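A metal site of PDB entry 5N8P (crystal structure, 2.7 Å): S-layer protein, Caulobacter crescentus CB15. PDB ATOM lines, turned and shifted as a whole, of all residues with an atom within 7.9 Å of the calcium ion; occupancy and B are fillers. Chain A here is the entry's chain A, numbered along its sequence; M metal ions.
The backbone NH (N) of Thr 897 lies within hydrogen-bond range of the backbone carbonyl oxygen (O) of Asp 878, 2.8 Å away. The backbone NH (N) of Ser 873 sits close to the side-chain hydroxyl (OG1) of Thr 892 (3.4 Å). N of Ala 874 lies within hydrogen-bond range of OG1 of Thr 892 (3.3 Å).
Thr 892 touches the calcium ion. Within 4 Å of the calcium ion: Ser 873, Ala 876, Asp 878, Thr 892, Gly 893 and Asp 896. The nearest printed residue that does not touch the calcium ion is Ala 874 (4.3 Å).
The calcium ion is bound by O of Gly 893, OD2 of Asp 878, O of Ser 873, OD2 of Asp 896, O of Ala 876 and OD1 of Asp 896. The calcium ion has six donor atoms within binding distance.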
ATOM      1  N   GLU A 857      -4.606   4.927 -17.579  1.00  0.00           N
ATOM      2  CA  GLU A 857      -3.893   3.906 -18.351  1.00  0.00           C
ATOM      3  C   GLU A 857      -4.758   3.022 -19.261  1.00  0.00           C
ATOM      4  O   GLU A 857      -5.915   2.723 -18.936  1.00  0.00           O
ATOM      5  CB  GLU A 857      -3.048   3.018 -17.453  1.00  0.00           C
ATOM      6  CG  GLU A 857      -1.558   3.305 -17.562  1.00  0.00           C
ATOM      7  CD  GLU A 857      -0.909   3.023 -18.917  1.00  0.00           C
ATOM      8  OE1 GLU A 857      -1.571   2.772 -19.961  1.00  0.00           O
ATOM      9  OE2 GLU A 857       0.324   3.044 -18.921  1.00  0.00           O
ATOM     10  N   VAL A 859      -4.889  -0.643 -20.253  1.00  0.00           N
ATOM     11  CA  VAL A 859      -4.490  -1.994 -19.804  1.00  0.00           C
ATOM     12  C   VAL A 859      -5.242  -3.045 -20.641  1.00  0.00           C
ATOM     13  O   VAL A 859      -6.442  -2.974 -20.773  1.00  0.00           O
ATOM     14  CB  VAL A 859      -4.825  -2.205 -18.282  1.00  0.00           C
ATOM     15  CG1 VAL A 859      -4.583  -3.627 -17.842  1.00  0.00           C
ATOM     16  CG2 VAL A 859      -4.005  -1.290 -17.394  1.00  0.00           C
ATOM     17  N   ILE A 861      -6.236  -7.023 -20.932  1.00  0.00           N
ATOM     18  CA  ILE A 861      -6.313  -8.332 -20.271  1.00  0.00           C
ATOM     19  C   ILE A 861      -6.988  -9.428 -21.136  1.00  0.00           C
ATOM     20  O   ILE A 861      -8.169  -9.355 -21.445  1.00  0.00           O
ATOM     21  CB  ILE A 861      -7.040  -8.217 -18.908  1.00  0.00           C
ATOM     22  CG1 ILE A 861      -6.426  -7.120 -18.033  1.00  0.00           C
ATOM     23  CG2 ILE A 861      -7.034  -9.560 -18.189  1.00  0.00           C
ATOM     24  CD1 ILE A 861      -7.227  -6.745 -16.814  1.00  0.00           C
ATOM     25  N   THR A 871      -9.913  -9.439 -13.600  1.00  0.00           N
ATOM     26  CA  THR A 871     -10.312  -8.176 -12.973  1.00  0.00           C
ATOM     27  C   THR A 871      -9.385  -7.058 -13.416  1.00  0.00           C
ATOM     28  O   THR A 871      -8.148  -7.234 -13.401  1.00  0.00           O
ATOM     29  CB  THR A 871     -10.329  -8.316 -11.440  1.00  0.00           C
ATOM     30  OG1 THR A 871     -11.307  -9.283 -11.056  1.00  0.00           O
ATOM     31  CG2 THR A 871     -10.646  -6.993 -10.710  1.00  0.00           C
ATOM     32  N   GLY A 872      -9.953  -5.903 -13.797  1.00  0.00           N
ATOM     33  CA  GLY A 872      -9.165  -4.717 -14.141  1.00  0.00           C
ATOM     34  C   GLY A 872      -8.789  -3.884 -12.917  1.00  0.00           C
ATOM     35  O   GLY A 872      -8.687  -4.400 -11.783  1.00  0.00           O
ATOM     36  N   SER A 873      -8.588  -2.591 -13.154  1.00  0.00           N
ATOM     37  CA  SER A 873      -8.198  -1.619 -12.137  1.00  0.00           C
ATOM     38  C   SER A 873      -9.233  -0.508 -12.209  1.00  0.00           C
ATOM     39  O   SER A 873      -9.684  -0.153 -13.313  1.00  0.00           O
ATOM     40  CB  SER A 873      -6.820  -1.016 -12.447  1.00  0.00           C
ATOM     41  OG  SER A 873      -6.067  -1.778 -13.409  1.00  0.00           O
ATOM     42  N   ALA A 874      -9.621   0.061 -11.069  1.00  0.00           N
ATOM     43  CA  ALA A 874     -10.458   1.292 -11.073  1.00  0.00           C
ATOM     44  C   ALA A 874      -9.789   2.480 -11.783  1.00  0.00           C
ATOM     45  O   ALA A 874     -10.445   3.363 -12.312  1.00  0.00           O
ATOM     46  CB  ALA A 874     -10.835   1.681  -9.645  1.00  0.00           C
ATOM     47  N   THR A 875      -8.462   2.461 -11.757  1.00  0.00           N
ATOM     48  CA  THR A 875      -7.601   3.474 -12.321  1.00  0.00           C
ATOM     49  C   THR A 875      -7.643   3.484 -13.859  1.00  0.00           C
ATOM     50  O   THR A 875      -7.254   4.465 -14.495  1.00  0.00           O
ATOM     51  CB  THR A 875      -6.164   3.145 -11.815  1.00  0.00           C
ATOM     52  OG1 THR A 875      -5.529   4.363 -11.464  1.00  0.00           O
ATOM     53  CG2 THR A 875      -5.273   2.365 -12.833  1.00  0.00           C
ATOM     54  N   ALA A 876      -8.092   2.383 -14.461  1.00  0.00           N
ATOM     55  CA  ALA A 876      -7.681   2.092 -15.811  1.00  0.00           C
ATOM     56  C   ALA A 876      -8.813   1.842 -16.771  1.00  0.00           C
ATOM     57  O   ALA A 876      -9.889   1.365 -16.403  1.00  0.00           O
ATOM     58  CB  ALA A 876      -6.736   0.910 -15.832  1.00  0.00           C
ATOM     59  N   ASN A 877      -8.490   2.145 -18.015  1.00  0.00           N
ATOM     60  CA  ASN A 877      -9.337   1.867 -19.140  1.00  0.00           C
ATOM     61  C   ASN A 877      -8.985   0.463 -19.657  1.00  0.00           C
ATOM     62  O   ASN A 877      -8.285   0.324 -20.668  1.00  0.00           O
ATOM     63  CB  ASN A 877      -9.116   2.940 -20.220  1.00  0.00           C
ATOM     64  CG  ASN A 877      -9.668   4.310 -19.851  1.00  0.00           C
ATOM     65  OD1 ASN A 877     -10.306   4.512 -18.800  1.00  0.00           O
ATOM     66  ND2 ASN A 877      -9.482   5.250 -20.745  1.00  0.00           N
ATOM     67  N   ASP A 878      -9.502  -0.548 -18.952  1.00  0.00           N
ATOM     68  CA  ASP A 878      -9.225  -1.967 -19.224  1.00  0.00           C
ATOM     69  C   ASP A 878     -10.005  -2.495 -20.425  1.00  0.00           C
ATOM     70  O   ASP A 878     -11.222  -2.376 -20.497  1.00  0.00           O
ATOM     71  CB  ASP A 878      -9.512  -2.845 -18.001  1.00  0.00           C
ATOM     72  CG  ASP A 878      -8.862  -2.320 -16.683  1.00  0.00           C
ATOM     73  OD1 ASP A 878      -7.640  -2.557 -16.433  1.00  0.00           O
ATOM     74  OD2 ASP A 878      -9.628  -1.724 -15.886  1.00  0.00           O
ATOM     75  N   THR A 879      -9.283  -3.063 -21.383  1.00  0.00           N
ATOM     76  CA  THR A 879      -9.861  -3.936 -22.411  1.00  0.00           C
ATOM     77  C   THR A 879      -9.714  -5.378 -21.914  1.00  0.00           C
ATOM     78  O   THR A 879      -8.585  -5.872 -21.827  1.00  0.00           O
ATOM     79  CB  THR A 879      -9.154  -3.769 -23.762  1.00  0.00           C
ATOM     80  OG1 THR A 879      -9.201  -2.401 -24.133  1.00  0.00           O
ATOM     81  CG2 THR A 879      -9.866  -4.550 -24.855  1.00  0.00           C
ATOM     82  N   ILE A 880     -10.825  -6.026 -21.566  1.00  0.00           N
ATOM     83  CA  ILE A 880     -10.779  -7.391 -21.055  1.00  0.00           C
ATOM     84  C   ILE A 880     -11.456  -8.343 -22.026  1.00  0.00           C
ATOM     85  O   ILE A 880     -12.550  -8.069 -22.454  1.00  0.00           O
ATOM     86  CB  ILE A 880     -11.378  -7.510 -19.633  1.00  0.00           C
ATOM     87  CG1 ILE A 880     -10.754  -6.457 -18.701  1.00  0.00           C
ATOM     88  CG2 ILE A 880     -11.127  -8.905 -19.098  1.00  0.00           C
ATOM     89  CD1 ILE A 880     -11.236  -6.452 -17.264  1.00  0.00           C
ATOM     90  N   VAL A 890     -14.501  -8.502 -14.535  1.00  0.00           N
ATOM     91  CA  VAL A 890     -14.884  -7.575 -13.456  1.00  0.00           C
ATOM     92  C   VAL A 890     -14.641  -6.075 -13.742  1.00  0.00           C
ATOM     93  O   VAL A 890     -13.539  -5.638 -14.125  1.00  0.00           O
ATOM     94  CB  VAL A 890     -14.304  -8.013 -12.095  1.00  0.00           C
ATOM     95  CG1 VAL A 890     -14.935  -7.245 -10.941  1.00  0.00           C
ATOM     96  CG2 VAL A 890     -14.589  -9.488 -11.883  1.00  0.00           C
ATOM     97  N   TYR A 891     -15.699  -5.292 -13.549  1.00  0.00           N
ATOM     98  CA  TYR A 891     -15.611  -3.857 -13.671  1.00  0.00           C
ATOM     99  C   TYR A 891     -15.385  -3.193 -12.325  1.00  0.00           C
ATOM    100  O   TYR A 891     -16.116  -3.430 -11.335  1.00  0.00           O
ATOM    101  CB  TYR A 891     -16.854  -3.297 -14.372  1.00  0.00           C
ATOM    102  CG  TYR A 891     -16.800  -1.806 -14.614  1.00  0.00           C
ATOM    103  CD1 TYR A 891     -15.828  -1.240 -15.447  1.00  0.00           C
ATOM    104  CD2 TYR A 891     -17.726  -0.944 -14.003  1.00  0.00           C
ATOM    105  CE1 TYR A 891     -15.768   0.138 -15.664  1.00  0.00           C
ATOM    106  CE2 TYR A 891     -17.660   0.440 -14.209  1.00  0.00           C
ATOM    107  CZ  TYR A 891     -16.691   0.969 -15.046  1.00  0.00           C
ATOM    108  OH  TYR A 891     -16.648   2.331 -15.255  1.00  0.00           O
ATOM    109  N   THR A 892     -14.374  -2.323 -12.310  1.00  0.00           N
ATOM    110  CA  THR A 892     -13.913  -1.628 -11.093  1.00  0.00           C
ATOM    111  C   THR A 892     -13.990  -0.107 -11.193  1.00  0.00           C
ATOM    112  O   THR A 892     -14.009   0.558 -10.160  1.00  0.00           O
ATOM    113  CB  THR A 892     -12.446  -1.970 -10.823  1.00  0.00           C
ATOM    114  OG1 THR A 892     -11.763  -2.189 -12.071  1.00  0.00           O
ATOM    115  CG2 THR A 892     -12.348  -3.192  -9.935  1.00  0.00           C
ATOM    116  N   GLY A 893     -14.013   0.417 -12.431  1.00  0.00           N
ATOM    117  CA  GLY A 893     -14.031   1.868 -12.669  1.00  0.00           C
ATOM    118  C   GLY A 893     -13.377   2.192 -13.995  1.00  0.00           C
ATOM    119  O   GLY A 893     -12.605   1.380 -14.508  1.00  0.00           O
ATOM    120  N   GLY A 894     -13.704   3.365 -14.554  1.00  0.00           N
ATOM    121  CA  GLY A 894     -13.087   3.876 -15.791  1.00  0.00           C
ATOM    122  C   GLY A 894     -13.693   3.366 -17.086  1.00  0.00           C
ATOM    123  O   GLY A 894     -14.694   2.668 -17.078  1.00  0.00           O
ATOM    124  N   THR A 895     -13.095   3.726 -18.213  1.00  0.00           N
ATOM    125  CA  THR A 895     -13.703   3.392 -19.490  1.00  0.00           C
ATOM    126  C   THR A 895     -13.236   1.996 -19.927  1.00  0.00           C
ATOM    127  O   THR A 895     -12.178   1.835 -20.527  1.00  0.00           O
ATOM    128  CB  THR A 895     -13.483   4.520 -20.540  1.00  0.00           C
ATOM    129  OG1 THR A 895     -13.953   5.758 -19.997  1.00  0.00           O
ATOM    130  CG2 THR A 895     -14.230   4.251 -21.857  1.00  0.00           C
ATOM    131  N   ASP A 896     -14.060   0.988 -19.621  1.00  0.00           N
ATOM    132  CA  ASP A 896     -13.691  -0.412 -19.885  1.00  0.00           C
ATOM    133  C   ASP A 896     -14.400  -1.035 -21.085  1.00  0.00           C
ATOM    134  O   ASP A 896     -15.558  -0.762 -21.342  1.00  0.00           O
ATOM    135  CB  ASP A 896     -13.883  -1.270 -18.623  1.00  0.00           C
ATOM    136  CG  ASP A 896     -12.775  -1.026 -17.551  1.00  0.00           C
ATOM    137  OD1 ASP A 896     -11.857  -0.189 -17.746  1.00  0.00           O
ATOM    138  OD2 ASP A 896     -12.807  -1.685 -16.467  1.00  0.00           O
ATOM    139  N   THR A 897     -13.692  -1.891 -21.806  1.00  0.00           N
ATOM    140  CA  THR A 897     -14.247  -2.614 -22.954  1.00  0.00           C
ATOM    141  C   THR A 897     -14.155  -4.155 -22.736  1.00  0.00           C
ATOM    142  O   THR A 897     -13.062  -4.739 -22.731  1.00  0.00           O
ATOM    143  CB  THR A 897     -13.543  -2.139 -24.239  1.00  0.00           C
ATOM    144  OG1 THR A 897     -13.728  -0.731 -24.365  1.00  0.00           O
ATOM    145  CG2 THR A 897     -14.050  -2.858 -25.500  1.00  0.00           C
ATOM    146  N   PHE A 898     -15.309  -4.775 -22.550  1.00  0.00           N
ATOM    147  CA  PHE A 898     -15.447  -6.200 -22.242  1.00  0.00           C
ATOM    148  C   PHE A 898     -15.926  -7.000 -23.444  1.00  0.00           C
ATOM    149  O   PHE A 898     -16.838  -6.604 -24.168  1.00  0.00           O
ATOM    150  CB  PHE A 898     -16.441  -6.418 -21.111  1.00  0.00           C
ATOM    151  CG  PHE A 898     -15.925  -6.036 -19.746  1.00  0.00           C
ATOM    152  CD1 PHE A 898     -16.693  -6.315 -18.609  1.00  0.00           C
ATOM    153  CD2 PHE A 898     -14.697  -5.424 -19.560  1.00  0.00           C
ATOM    154  CE1 PHE A 898     -16.254  -5.987 -17.335  1.00  0.00           C
ATOM    155  CE2 PHE A 898     -14.253  -5.082 -18.287  1.00  0.00           C
ATOM    156  CZ  PHE A 898     -15.029  -5.383 -17.170  1.00  0.00           C
ATOM    157  N   ALA A 911     -18.579  -1.611  -9.882  1.00  0.00           N
ATOM    158  CA  ALA A 911     -18.539  -0.162  -9.743  1.00  0.00           C
ATOM    159  C   ALA A 911     -19.621   0.580 -10.543  1.00  0.00           C
ATOM    160  O   ALA A 911     -20.205   0.071 -11.507  1.00  0.00           O
ATOM    161  CB  ALA A 911     -17.155   0.353 -10.086  1.00  0.00           C
ATOM    162  N   VAL A 919     -18.600   0.959 -18.496  1.00  0.00           N
ATOM    163  CA  VAL A 919     -18.276  -0.268 -19.222  1.00  0.00           C
ATOM    164  C   VAL A 919     -19.123  -0.458 -20.483  1.00  0.00           C
ATOM    165  O   VAL A 919     -20.342  -0.315 -20.454  1.00  0.00           O
ATOM    166  CB  VAL A 919     -18.298  -1.502 -18.287  1.00  0.00           C
ATOM    167  CG1 VAL A 919     -19.563  -1.532 -17.429  1.00  0.00           C
ATOM    168  CG2 VAL A 919     -18.098  -2.799 -19.063  1.00  0.00           C
HETATM  169 CA    CA M   1     -11.334  -0.371 -15.044  1.00  0.00          CA
